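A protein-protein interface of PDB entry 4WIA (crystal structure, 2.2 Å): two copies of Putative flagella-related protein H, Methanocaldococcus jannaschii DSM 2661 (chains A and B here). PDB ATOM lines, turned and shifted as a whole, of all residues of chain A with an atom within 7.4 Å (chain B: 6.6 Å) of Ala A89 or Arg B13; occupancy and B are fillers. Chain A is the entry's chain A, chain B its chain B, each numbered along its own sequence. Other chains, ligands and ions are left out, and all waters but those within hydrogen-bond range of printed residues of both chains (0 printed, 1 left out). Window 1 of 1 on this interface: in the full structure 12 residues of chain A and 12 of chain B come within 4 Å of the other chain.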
ATOM      1  N   LEU A  52     -26.104  12.293 -20.896  1.00  0.00           N
ATOM      2  CA  LEU A  52     -24.756  12.051 -21.373  1.00  0.00           C
ATOM      3  C   LEU A  52     -24.487  10.573 -21.670  1.00  0.00           C
ATOM      4  O   LEU A  52     -23.828  10.235 -22.656  1.00  0.00           O
ATOM      5  CB  LEU A  52     -23.732  12.545 -20.364  1.00  0.00           C
ATOM      6  CG  LEU A  52     -23.623  14.046 -20.246  1.00  0.00           C
ATOM      7  CD1 LEU A  52     -22.905  14.389 -18.956  1.00  0.00           C
ATOM      8  CD2 LEU A  52     -22.848  14.596 -21.439  1.00  0.00           C
ATOM      9  N   ARG A  55     -25.802   9.457 -25.025  1.00  0.00           N
ATOM     10  CA  ARG A  55     -25.164  10.056 -26.221  1.00  0.00           C
ATOM     11  C   ARG A  55     -25.757  11.407 -26.617  1.00  0.00           C
ATOM     12  O   ARG A  55     -25.627  11.821 -27.755  1.00  0.00           O
ATOM     13  CB  ARG A  55     -25.179   9.107 -27.419  1.00  0.00           C
ATOM     14  CG  ARG A  55     -24.645   7.702 -27.127  1.00  0.00           C
ATOM     15  CD  ARG A  55     -23.180   7.759 -26.742  1.00  0.00           C
ATOM     16  NE  ARG A  55     -22.734   6.479 -26.275  1.00  0.00           N
ATOM     17  CZ  ARG A  55     -21.474   6.143 -25.987  1.00  0.00           C
ATOM     18  NH1 ARG A  55     -21.237   4.931 -25.514  1.00  0.00           N
ATOM     19  NH2 ARG A  55     -20.455   6.939 -26.211  1.00  0.00           N
ATOM     20  N   TYR A  56     -26.355  12.094 -25.650  1.00  0.00           N
ATOM     21  CA  TYR A  56     -26.660  13.522 -25.779  1.00  0.00           C
ATOM     22  C   TYR A  56     -25.519  14.418 -25.191  1.00  0.00           C
ATOM     23  O   TYR A  56     -24.663  13.953 -24.456  1.00  0.00           O
ATOM     24  CB  TYR A  56     -27.979  13.853 -25.111  1.00  0.00           C
ATOM     25  CG  TYR A  56     -29.140  13.034 -25.641  1.00  0.00           C
ATOM     26  CD1 TYR A  56     -29.838  13.448 -26.759  1.00  0.00           C
ATOM     27  CD2 TYR A  56     -29.514  11.832 -25.038  1.00  0.00           C
ATOM     28  CE1 TYR A  56     -30.884  12.721 -27.270  1.00  0.00           C
ATOM     29  CE2 TYR A  56     -30.558  11.081 -25.537  1.00  0.00           C
ATOM     30  CZ  TYR A  56     -31.235  11.523 -26.644  1.00  0.00           C
ATOM     31  OH  TYR A  56     -32.267  10.859 -27.138  1.00  0.00           O
ATOM     32  N   SER A  57     -25.484  15.682 -25.611  1.00  0.00           N
ATOM     33  CA  SER A  57     -24.538  16.623 -25.089  1.00  0.00           C
ATOM     34  C   SER A  57     -25.276  17.538 -24.124  1.00  0.00           C
ATOM     35  O   SER A  57     -26.451  17.738 -24.277  1.00  0.00           O
ATOM     36  CB  SER A  57     -23.924  17.438 -26.202  1.00  0.00           C
ATOM     37  OG  SER A  57     -24.925  18.073 -27.004  1.00  0.00           O
ATOM     38  N   VAL A  58     -24.576  18.035 -23.105  1.00  0.00           N
ATOM     39  CA  VAL A  58     -25.171  18.840 -22.098  1.00  0.00           C
ATOM     40  C   VAL A  58     -24.294  20.071 -21.823  1.00  0.00           C
ATOM     41  O   VAL A  58     -23.071  19.954 -21.735  1.00  0.00           O
ATOM     42  CB  VAL A  58     -25.321  18.030 -20.800  1.00  0.00           C
ATOM     43  CG1 VAL A  58     -25.874  18.901 -19.691  1.00  0.00           C
ATOM     44  CG2 VAL A  58     -26.246  16.849 -21.012  1.00  0.00           C
ATOM     45  N   THR A  59     -24.936  21.218 -21.627  1.00  0.00           N
ATOM     46  CA  THR A  59     -24.335  22.345 -20.998  1.00  0.00           C
ATOM     47  C   THR A  59     -24.910  22.494 -19.602  1.00  0.00           C
ATOM     48  O   THR A  59     -26.146  22.514 -19.429  1.00  0.00           O
ATOM     49  CB  THR A  59     -24.641  23.645 -21.760  1.00  0.00           C
ATOM     50  OG1 THR A  59     -23.988  23.595 -23.027  1.00  0.00           O
ATOM     51  CG2 THR A  59     -24.105  24.899 -21.000  1.00  0.00           C
ATOM     52  N   LYS A  83     -14.525  12.056 -18.437  1.00  0.00           N
ATOM     53  CA  LYS A  83     -14.331  11.870 -19.861  1.00  0.00           C
ATOM     54  C   LYS A  83     -15.252  12.723 -20.700  1.00  0.00           C
ATOM     55  O   LYS A  83     -14.864  13.150 -21.797  1.00  0.00           O
ATOM     56  CB  LYS A  83     -14.443  10.417 -20.282  1.00  0.00           C
ATOM     57  CG  LYS A  83     -13.149   9.692 -20.014  1.00  0.00           C
ATOM     58  CD  LYS A  83     -13.028   8.429 -20.824  1.00  0.00           C
ATOM     59  CE  LYS A  83     -11.582   7.984 -20.883  1.00  0.00           C
ATOM     60  NZ  LYS A  83     -11.471   6.713 -21.646  1.00  0.00           N
ATOM     61  N   LYS A  84     -16.444  12.966 -20.211  1.00  0.00           N
ATOM     62  CA  LYS A  84     -17.401  13.747 -20.947  1.00  0.00           C
ATOM     63  C   LYS A  84     -16.950  15.226 -20.959  1.00  0.00           C
ATOM     64  O   LYS A  84     -17.122  15.905 -21.964  1.00  0.00           O
ATOM     65  CB  LYS A  84     -18.783  13.624 -20.329  1.00  0.00           C
ATOM     66  CG  LYS A  84     -19.395  12.218 -20.372  1.00  0.00           C
ATOM     67  CD  LYS A  84     -19.835  11.857 -21.776  1.00  0.00           C
ATOM     68  CE  LYS A  84     -20.455  10.487 -21.844  1.00  0.00           C
ATOM     69  NZ  LYS A  84     -21.005  10.189 -23.207  1.00  0.00           N
ATOM     70  N   LEU A  85     -16.331  15.689 -19.865  1.00  0.00           N
ATOM     71  CA  LEU A  85     -15.712  17.002 -19.850  1.00  0.00           C
ATOM     72  C   LEU A  85     -14.588  17.102 -20.858  1.00  0.00           C
ATOM     73  O   LEU A  85     -14.453  18.145 -21.545  1.00  0.00           O
ATOM     74  CB  LEU A  85     -15.179  17.376 -18.473  1.00  0.00           C
ATOM     75  CG  LEU A  85     -16.211  17.834 -17.437  1.00  0.00           C
ATOM     76  CD1 LEU A  85     -15.552  17.848 -16.053  1.00  0.00           C
ATOM     77  CD2 LEU A  85     -16.838  19.197 -17.767  1.00  0.00           C
ATOM     78  N   LEU A  86     -13.757  16.070 -20.928  1.00  0.00           N
ATOM     79  CA  LEU A  86     -12.553  16.151 -21.753  1.00  0.00           C
ATOM     80  C   LEU A  86     -12.883  16.192 -23.208  1.00  0.00           C
ATOM     81  O   LEU A  86     -12.149  16.761 -23.978  1.00  0.00           O
ATOM     82  CB  LEU A  86     -11.600  14.996 -21.469  1.00  0.00           C
ATOM     83  CG  LEU A  86     -10.906  15.058 -20.096  1.00  0.00           C
ATOM     84  CD1 LEU A  86     -10.196  13.759 -19.746  1.00  0.00           C
ATOM     85  CD2 LEU A  86      -9.932  16.201 -20.022  1.00  0.00           C
ATOM     86  N   SER A  87     -14.001  15.612 -23.601  1.00  0.00           N
ATOM     87  CA  SER A  87     -14.362  15.534 -25.013  1.00  0.00           C
ATOM     88  C   SER A  87     -15.180  16.748 -25.428  1.00  0.00           C
ATOM     89  O   SER A  87     -15.433  16.966 -26.624  1.00  0.00           O
ATOM     90  CB  SER A  87     -15.158  14.253 -25.289  1.00  0.00           C
ATOM     91  OG  SER A  87     -16.394  14.308 -24.624  1.00  0.00           O
ATOM     92  N   GLY A  88     -15.604  17.536 -24.443  1.00  0.00           N
ATOM     93  CA  GLY A  88     -16.581  18.562 -24.701  1.00  0.00           C
ATOM     94  C   GLY A  88     -18.033  18.103 -24.775  1.00  0.00           C
ATOM     95  O   GLY A  88     -18.930  18.938 -24.897  1.00  0.00           O
ATOM     96  N   ALA A  89     -18.303  16.803 -24.639  1.00  0.00           N
ATOM     97  CA  ALA A  89     -19.640  16.327 -24.480  1.00  0.00           C
ATOM     98  C   ALA A  89     -20.412  17.014 -23.378  1.00  0.00           C
ATOM     99  O   ALA A  89     -21.617  17.370 -23.576  1.00  0.00           O
ATOM    100  CB  ALA A  89     -19.639  14.858 -24.238  1.00  0.00           C
ATOM    101  N   LEU A  90     -19.751  17.251 -22.263  1.00  0.00           N
ATOM    102  CA  LEU A  90     -20.299  18.099 -21.188  1.00  0.00           C
ATOM    103  C   LEU A  90     -19.531  19.428 -21.144  1.00  0.00           C
ATOM    104  O   LEU A  90     -18.313  19.443 -21.022  1.00  0.00           O
ATOM    105  CB  LEU A  90     -20.163  17.393 -19.836  1.00  0.00           C
ATOM    106  CG  LEU A  90     -20.481  18.201 -18.567  1.00  0.00           C
ATOM    107  CD1 LEU A  90     -21.882  18.766 -18.652  1.00  0.00           C
ATOM    108  CD2 LEU A  90     -20.318  17.415 -17.268  1.00  0.00           C
ATOM    109  N   LEU A  91     -20.256  20.565 -21.257  1.00  0.00           N
ATOM    110  CA  LEU A  91     -19.687  21.866 -21.137  1.00  0.00           C
ATOM    111  C   LEU A  91     -20.211  22.417 -19.844  1.00  0.00           C
ATOM    112  O   LEU A  91     -21.423  22.626 -19.659  1.00  0.00           O
ATOM    113  CB  LEU A  91     -20.168  22.752 -22.304  1.00  0.00           C
ATOM    114  CG  LEU A  91     -19.892  24.230 -22.279  1.00  0.00           C
ATOM    115  CD1 LEU A  91     -18.374  24.489 -22.310  1.00  0.00           C
ATOM    116  CD2 LEU A  91     -20.602  24.928 -23.429  1.00  0.00           C
ATOM    117  N   TYR A  92     -19.289  22.635 -18.916  1.00  0.00           N
ATOM    118  CA  TYR A  92     -19.619  23.071 -17.577  1.00  0.00           C
ATOM    119  C   TYR A  92     -19.232  24.547 -17.400  1.00  0.00           C
ATOM    120  O   TYR A  92     -18.111  24.913 -17.630  1.00  0.00           O
ATOM    121  CB  TYR A  92     -18.883  22.204 -16.526  1.00  0.00           C
ATOM    122  CG  TYR A  92     -19.311  22.557 -15.138  1.00  0.00           C
ATOM    123  CD1 TYR A  92     -20.526  22.143 -14.664  1.00  0.00           C
ATOM    124  CD2 TYR A  92     -18.568  23.420 -14.348  1.00  0.00           C
ATOM    125  CE1 TYR A  92     -20.964  22.508 -13.400  1.00  0.00           C
ATOM    126  CE2 TYR A  92     -18.992  23.800 -13.067  1.00  0.00           C
ATOM    127  CZ  TYR A  92     -20.205  23.319 -12.608  1.00  0.00           C
ATOM    128  OH  TYR A  92     -20.650  23.681 -11.356  1.00  0.00           O
ATOM    129  N   LYS A 121     -25.282  22.553 -27.494  1.00  0.00           N
ATOM    130  CA  LYS A 121     -25.554  21.232 -26.917  1.00  0.00           C
ATOM    131  C   LYS A 121     -27.017  20.907 -26.950  1.00  0.00           C
ATOM    132  O   LYS A 121     -27.831  21.796 -27.254  1.00  0.00           O
ATOM    133  CB  LYS A 121     -25.051  21.155 -25.470  1.00  0.00           C
ATOM    134  CG  LYS A 121     -23.617  21.573 -25.267  1.00  0.00           C
ATOM    135  CD  LYS A 121     -22.701  20.892 -26.251  1.00  0.00           C
ATOM    136  CE  LYS A 121     -21.266  21.015 -25.786  1.00  0.00           C
ATOM    137  NZ  LYS A 121     -20.342  20.590 -26.872  1.00  0.00           N
ATOM    138  N   ASP A 122     -27.363  19.618 -26.694  1.00  0.00           N
ATOM    139  CA  ASP A 122     -28.758  19.151 -26.788  1.00  0.00           C
ATOM    140  C   ASP A 122     -29.540  19.643 -25.626  1.00  0.00           C
ATOM    141  O   ASP A 122     -30.719  19.934 -25.745  1.00  0.00           O
ATOM    142  CB  ASP A 122     -28.853  17.641 -26.849  1.00  0.00           C
ATOM    143  CG  ASP A 122     -28.085  17.055 -28.009  1.00  0.00           C
ATOM    144  OD1 ASP A 122     -28.203  17.598 -29.138  1.00  0.00           O
ATOM    145  OD2 ASP A 122     -27.323  16.090 -27.767  1.00  0.00           O
ATOM    146  N   VAL A 123     -28.900  19.799 -24.497  1.00  0.00           N
ATOM    147  CA  VAL A 123     -29.600  20.062 -23.271  1.00  0.00           C
ATOM    148  C   VAL A 123     -28.864  21.145 -22.569  1.00  0.00           C
ATOM    149  O   VAL A 123     -27.654  21.028 -22.406  1.00  0.00           O
ATOM    150  CB  VAL A 123     -29.589  18.800 -22.358  1.00  0.00           C
ATOM    151  CG1 VAL A 123     -30.282  19.073 -21.043  1.00  0.00           C
ATOM    152  CG2 VAL A 123     -30.285  17.624 -23.049  1.00  0.00           C
ATOM    153  N   ASP B  10     -23.706   7.617 -33.086  1.00  0.00           N
ATOM    154  CA  ASP B  10     -23.887   8.713 -32.145  1.00  0.00           C
ATOM    155  C   ASP B  10     -22.825   8.757 -31.058  1.00  0.00           C
ATOM    156  O   ASP B  10     -22.599   7.725 -30.356  1.00  0.00           O
ATOM    157  CB  ASP B  10     -25.223   8.559 -31.350  1.00  0.00           C
ATOM    158  CG  ASP B  10     -26.400   8.299 -32.208  1.00  0.00           C
ATOM    159  OD1 ASP B  10     -26.300   7.570 -33.215  1.00  0.00           O
ATOM    160  OD2 ASP B  10     -27.440   8.881 -31.903  1.00  0.00           O
ATOM    161  N   LEU B  11     -22.286   9.960 -30.829  1.00  0.00           N
ATOM    162  CA  LEU B  11     -21.533  10.278 -29.651  1.00  0.00           C
ATOM    163  C   LEU B  11     -22.032  11.567 -28.992  1.00  0.00           C
ATOM    164  O   LEU B  11     -22.537  12.461 -29.653  1.00  0.00           O
ATOM    165  CB  LEU B  11     -20.089  10.419 -30.027  1.00  0.00           C
ATOM    166  CG  LEU B  11     -19.430   9.236 -30.716  1.00  0.00           C
ATOM    167  CD1 LEU B  11     -17.991   9.646 -30.977  1.00  0.00           C
ATOM    168  CD2 LEU B  11     -19.412   8.032 -29.816  1.00  0.00           C
ATOM    169  N   SER B  12     -21.891  11.666 -27.678  1.00  0.00           N
ATOM    170  CA  SER B  12     -22.297  12.858 -27.018  1.00  0.00           C
ATOM    171  C   SER B  12     -21.522  14.086 -27.578  1.00  0.00           C
ATOM    172  O   SER B  12     -22.075  15.199 -27.680  1.00  0.00           O
ATOM    173  CB  SER B  12     -22.021  12.754 -25.530  1.00  0.00           C
ATOM    174  OG  SER B  12     -22.881  11.915 -24.830  1.00  0.00           O
ATOM    175  N   ARG B  13     -20.248  13.892 -27.911  1.00  0.00           N
ATOM    176  CA  ARG B  13     -19.304  15.012 -28.143  1.00  0.00           C
ATOM    177  C   ARG B  13     -19.445  15.683 -29.481  1.00  0.00           C
ATOM    178  O   ARG B  13     -18.917  16.725 -29.672  1.00  0.00           O
ATOM    179  CB  ARG B  13     -17.869  14.518 -28.044  1.00  0.00           C
ATOM    180  CG  ARG B  13     -17.428  13.752 -29.274  1.00  0.00           C
ATOM    181  CD  ARG B  13     -16.087  13.155 -29.050  1.00  0.00           C
ATOM    182  NE  ARG B  13     -16.135  11.930 -28.264  1.00  0.00           N
ATOM    183  CZ  ARG B  13     -15.049  11.298 -27.817  1.00  0.00           C
ATOM    184  NH1 ARG B  13     -15.131  10.187 -27.083  1.00  0.00           N
ATOM    185  NH2 ARG B  13     -13.840  11.778 -28.085  1.00  0.00           N
ATOM    186  N   ASP B  14     -20.144  15.100 -30.426  1.00  0.00           N
ATOM    187  CA  ASP B  14     -20.398  15.811 -31.653  1.00  0.00           C
ATOM    188  C   ASP B  14     -21.777  15.449 -32.173  1.00  0.00           C
ATOM    189  O   ASP B  14     -22.473  14.612 -31.610  1.00  0.00           O
ATOM    190  CB  ASP B  14     -19.309  15.509 -32.662  1.00  0.00           C
ATOM    191  CG  ASP B  14     -19.311  14.071 -33.155  1.00  0.00           C
ATOM    192  OD1 ASP B  14     -20.371  13.551 -33.549  1.00  0.00           O
ATOM    193  OD2 ASP B  14     -18.207  13.466 -33.242  1.00  0.00           O
ATOM    194  N   ASP B  15     -22.189  16.098 -33.245  1.00  0.00           N
ATOM    195  CA  ASP B  15     -23.496  15.830 -33.835  1.00  0.00           C
ATOM    196  C   ASP B  15     -23.352  15.272 -35.210  1.00  0.00           C
ATOM    197  O   ASP B  15     -24.160  15.538 -36.088  1.00  0.00           O
ATOM    198  CB  ASP B  15     -24.340  17.119 -33.819  1.00  0.00           C
ATOM    199  CG  ASP B  15     -23.773  18.242 -34.742  1.00  0.00           C
ATOM    200  OD1 ASP B  15     -22.624  18.148 -35.237  1.00  0.00           O
ATOM    201  OD2 ASP B  15     -24.490  19.239 -34.935  1.00  0.00           O
ATOM    202  N   ARG B  46     -13.168   8.043 -36.109  1.00  0.00           N
ATOM    203  CA  ARG B  46     -14.426   8.532 -35.543  1.00  0.00           C
ATOM    204  C   ARG B  46     -15.577   7.598 -35.831  1.00  0.00           C
ATOM    205  O   ARG B  46     -16.402   7.281 -34.933  1.00  0.00           O
ATOM    206  CB  ARG B  46     -14.782   9.922 -36.102  1.00  0.00           C
ATOM    207  CG  ARG B  46     -16.248  10.349 -35.929  1.00  0.00           C
ATOM    208  CD  ARG B  46     -16.566  10.565 -34.460  1.00  0.00           C
ATOM    209  NE  ARG B  46     -17.949  10.973 -34.228  1.00  0.00           N
ATOM    210  CZ  ARG B  46     -18.997  10.143 -34.221  1.00  0.00           C
ATOM    211  NH1 ARG B  46     -18.848   8.845 -34.441  1.00  0.00           N
ATOM    212  NH2 ARG B  46     -20.219  10.636 -34.006  1.00  0.00           N
ATOM    213  N   TYR B  49     -15.127   4.356 -33.788  1.00  0.00           N
ATOM    214  CA  TYR B  49     -15.445   4.547 -32.394  1.00  0.00           C
ATOM    215  C   TYR B  49     -16.967   4.685 -32.185  1.00  0.00           C
ATOM    216  O   TYR B  49     -17.509   4.061 -31.242  1.00  0.00           O
ATOM    217  CB  TYR B  49     -14.732   5.724 -31.837  1.00  0.00           C
ATOM    218  CG  TYR B  49     -14.828   5.839 -30.360  1.00  0.00           C
ATOM    219  CD1 TYR B  49     -14.160   4.953 -29.512  1.00  0.00           C
ATOM    220  CD2 TYR B  49     -15.600   6.825 -29.788  1.00  0.00           C
ATOM    221  CE1 TYR B  49     -14.248   5.063 -28.161  1.00  0.00           C
ATOM    222  CE2 TYR B  49     -15.699   6.914 -28.422  1.00  0.00           C
ATOM    223  CZ  TYR B  49     -15.000   6.014 -27.627  1.00  0.00           C
ATOM    224  OH  TYR B  49     -15.079   6.182 -26.269  1.00  0.00           O
ATOM    225  N   LEU B  77      -6.960  10.811 -29.446  1.00  0.00           N
ATOM    226  CA  LEU B  77      -8.238  11.385 -29.801  1.00  0.00           C
ATOM    227  C   LEU B  77      -9.351  11.177 -28.766  1.00  0.00           C
ATOM    228  O   LEU B  77     -10.519  11.549 -28.986  1.00  0.00           O
ATOM    229  CB  LEU B  77      -8.656  10.805 -31.165  1.00  0.00           C
ATOM    230  CG  LEU B  77      -7.641  11.066 -32.307  1.00  0.00           C
ATOM    231  CD1 LEU B  77      -8.107  10.418 -33.587  1.00  0.00           C
ATOM    232  CD2 LEU B  77      -7.397  12.528 -32.561  1.00  0.00           C
ATOM    233  N   ASN B  78      -9.006  10.562 -27.635  1.00  0.00           N
ATOM    234  CA  ASN B  78     -10.000  10.156 -26.672  1.00  0.00           C
ATOM    235  C   ASN B  78     -11.043   9.229 -27.314  1.00  0.00           C
ATOM    236  O   ASN B  78     -12.244   9.315 -27.015  1.00  0.00           O
ATOM    237  CB  ASN B  78     -10.626  11.401 -26.043  1.00  0.00           C
ATOM    238  CG  ASN B  78     -11.649  11.066 -24.967  1.00  0.00           C
ATOM    239  OD1 ASN B  78     -11.864   9.904 -24.658  1.00  0.00           O
ATOM    240  ND2 ASN B  78     -12.322  12.100 -24.413  1.00  0.00           N
ATOM    241  N   TYR B  79     -10.597   8.372 -28.227  1.00  0.00           N
ATOM    242  CA  TYR B  79     -11.436   7.353 -28.767  1.00  0.00           C
ATOM    243  C   TYR B  79     -10.814   6.021 -28.294  1.00  0.00           C
ATOM    244  O   TYR B  79     -10.653   5.122 -29.098  1.00  0.00           O
ATOM    245  CB  TYR B  79     -11.421   7.307 -30.285  1.00  0.00           C
ATOM    246  CG  TYR B  79     -12.067   8.457 -31.035  1.00  0.00           C
ATOM    247  CD1 TYR B  79     -13.128   9.159 -30.516  1.00  0.00           C
ATOM    248  CD2 TYR B  79     -11.578   8.841 -32.283  1.00  0.00           C
ATOM    249  CE1 TYR B  79     -13.678  10.235 -31.222  1.00  0.00           C
ATOM    250  CE2 TYR B  79     -12.120   9.901 -33.005  1.00  0.00           C
ATOM    251  CZ  TYR B  79     -13.196  10.588 -32.484  1.00  0.00           C
ATOM    252  OH  TYR B  79     -13.731  11.684 -33.167  1.00  0.00           O
ATOM    253  N   SER B  80     -10.499   5.863 -27.009  1.00  0.00           N
ATOM    254  CA  SER B  80      -9.691   4.708 -26.631  1.00  0.00           C
ATOM    255  C   SER B  80     -10.475   3.373 -26.790  1.00  0.00           C
ATOM    256  O   SER B  80     -11.703   3.270 -26.537  1.00  0.00           O
ATOM    257  CB  SER B  80      -9.052   4.906 -25.254  1.00  0.00           C
ATOM    258  OG  SER B  80      -9.952   4.584 -24.258  1.00  0.00           O
ATOM    259  N   LYS B 222      -7.844  14.806 -27.685  1.00  0.00           N
ATOM    260  CA  LYS B 222      -8.866  14.269 -26.728  1.00  0.00           C
ATOM    261  C   LYS B 222     -10.321  14.611 -27.064  1.00  0.00           C
ATOM    262  O   LYS B 222     -11.244  14.527 -26.195  1.00  0.00           O
ATOM    263  CB  LYS B 222      -8.585  14.655 -25.250  1.00  0.00           C
ATOM    264  CG  LYS B 222      -7.248  14.193 -24.705  1.00  0.00           C
ATOM    265  CD  LYS B 222      -7.024  12.694 -24.884  1.00  0.00           C
ATOM    266  CE  LYS B 222      -7.095  11.968 -23.567  1.00  0.00           C
ATOM    267  NZ  LYS B 222      -7.393  10.520 -23.676  1.00  0.00           N
ATOM    268  N   ILE B 223     -10.510  14.981 -28.324  1.00  0.00           N
ATOM    269  CA  ILE B 223     -11.833  15.142 -28.891  1.00  0.00           C
ATOM    270  C   ILE B 223     -11.902  14.250 -30.117  1.00  0.00           C
ATOM    271  O   ILE B 223     -12.808  13.462 -30.266  1.00  0.00           O
ATOM    272  CB  ILE B 223     -12.104  16.623 -29.271  1.00  0.00           C
ATOM    273  CG1 ILE B 223     -12.099  17.502 -28.005  1.00  0.00           C
ATOM    274  CG2 ILE B 223     -13.409  16.753 -30.056  1.00  0.00           C
ATOM    275  CD1 ILE B 223     -12.179  18.991 -28.288  1.00  0.00           C
ATOM    276  N   GLY B 224     -10.916  14.392 -30.987  1.00  0.00           N
ATOM    277  CA  GLY B 224     -10.944  13.744 -32.276  1.00  0.00           C
ATOM    278  C   GLY B 224     -11.411  14.780 -33.289  1.00  0.00           C
ATOM    279  O   GLY B 224     -11.038  15.941 -33.203  1.00  0.00           O
ATOM    280  N   ILE B 225     -12.303  14.334 -34.161  1.00  0.00           N
ATOM    281  CA  ILE B 225     -13.017  15.180 -35.065  1.00  0.00           C
ATOM    282  C   ILE B 225     -13.854  16.161 -34.252  1.00  0.00           C
ATOM    283  O   ILE B 225     -14.759  15.758 -33.462  1.00  0.00           O
ATOM    284  CB  ILE B 225     -13.891  14.344 -36.006  1.00  0.00           C
ATOM    285  CG1 ILE B 225     -12.923  13.741 -37.066  1.00  0.00           C
ATOM    286  CG2 ILE B 225     -14.998  15.200 -36.632  1.00  0.00           C
ATOM    287  CD1 ILE B 225     -13.487  13.463 -38.434  1.00  0.00           C
ATOM    288  N   ALA B 226     -13.488  17.450 -34.402  1.00  0.00           N
ATOM    289  CA  ALA B 226     -14.224  18.555 -33.808  1.00  0.00           C
ATOM    290  C   ALA B 226     -14.934  19.189 -34.964  1.00  0.00           C
ATOM    291  O   ALA B 226     -14.318  19.875 -35.766  1.00  0.00           O
ATOM    292  CB  ALA B 226     -13.301  19.545 -33.129  1.00  0.00           C
ATOM    293  N   VAL B 227     -16.226  18.914 -35.059  1.00  0.00           N
ATOM    294  CA  VAL B 227     -17.049  19.384 -36.140  1.00  0.00           C
ATOM    295  C   VAL B 227     -17.405  20.828 -35.838  1.00  0.00           C
ATOM    296  O   VAL B 227     -17.777  21.157 -34.712  1.00  0.00           O
ATOM    297  CB  VAL B 227     -18.348  18.577 -36.247  1.00  0.00           C
ATOM    298  CG1 VAL B 227     -19.133  18.989 -37.487  1.00  0.00           C
ATOM    299  CG2 VAL B 227     -18.042  17.095 -36.316  1.00  0.00           C
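Of the 19 printed residues of chain A, 9 touch a printed residue of chain B.
Printed residues of chain A that touch a printed residue of chain B: Leu A52, Arg A55, Tyr A56, Ser A57, Lys A83, Lys A84, Leu A86, Ser A87 and Ala A89.
Among the printed residues, 16 pairs touch across the chains.
Among the printed residues, no Asp or Glu carboxylate lies within 4 Å of a Lys or Arg side-chain nitrogen of the other chain.
No position is printed for both chains.
Of the 16 pairs that touch across the chains among the printed residues, none has its exchanged pair printed and touching as well.
O of Asn B78 is in hydrogen-bond range of NH1 of Arg B13 (3.0 Å).
The backbone carbonyl oxygen (O) of Lys A84 sits at hydrogen-bond distance from the backbone NH (N) of Leu A90 (3.0 Å).
N of Val A58 is in hydrogen-bond range of O of Ala A89 (3.1 Å).
The backbone carbonyl oxygen (O) of Ser A57 is in hydrogen-bond range of the backbone NH (N) of Val A123, at 3.2 Å.
O of Ile B223 lies within hydrogen-bond range of NH2 of Arg B13 (2.9 Å).
The side-chain amino group (NZ) of Lys A84 lies within hydrogen-bond range of the backbone carbonyl oxygen (O) of Leu A52 (2.9 Å).
The backbone carbonyl oxygen (O) of Leu A52 sits at hydrogen-bond distance from the side-chain hydroxyl (OG) of Ser B12 (2.9 Å).
OG of Ser B12 sits at hydrogen-bond distance from NZ of Lys A84.
O of Lys B222 lies close to O of Leu A86 (3.3 Å).
OG of Ser B12 lies within hydrogen-bond range of O of Tyr A56, at 2.7 Å.
Of the printed residues of chain B, Arg A55 touches Asp B10 (3.7 Å), Leu B11 (3.7 Å) and Ser B12 (3.3 Å).
Printed residues of chain B within 4 Å of Leu A86: Lys B222.
Printed residues of chain B within 4 Å of Ala A89: Ser B12 and Arg B13.
Tyr B49 touches none of the printed residues of chain A.
Printed residues of chain A within 4 Å of Ile B223: Ser A87.
The nearest residue of chain A that does not touch Arg B13 is Gly A88 (4.7 Å).
The nearest printed residue of chain A that does not touch Lys B222 is Gly A88 (5.6 Å).
Arg A55 touches Leu B11.
Ser A57 touches Ser B12.
O of Lys A83 touches ND2 of Asn B78, at 3.8 Å.
OG of Ser B80 touches NZ of Lys A83, 3.7 Å away.
Arg B13 touches Ser A87 (CB to OG, 3.7 Å).
CB of Ser A87 touches ND2 of Asn B78, at 3.7 Å.
CA of Ser A87 touches O of Lys B222, 3.5 Å away.
CG1 of Ile B223 touches O of Ser A87, 3.6 Å away.
Ser B12 touches Ala A89 (CB to CB, 3.4 Å).
Ala A89 touches Arg B13 (CB to N, 3.8 Å).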
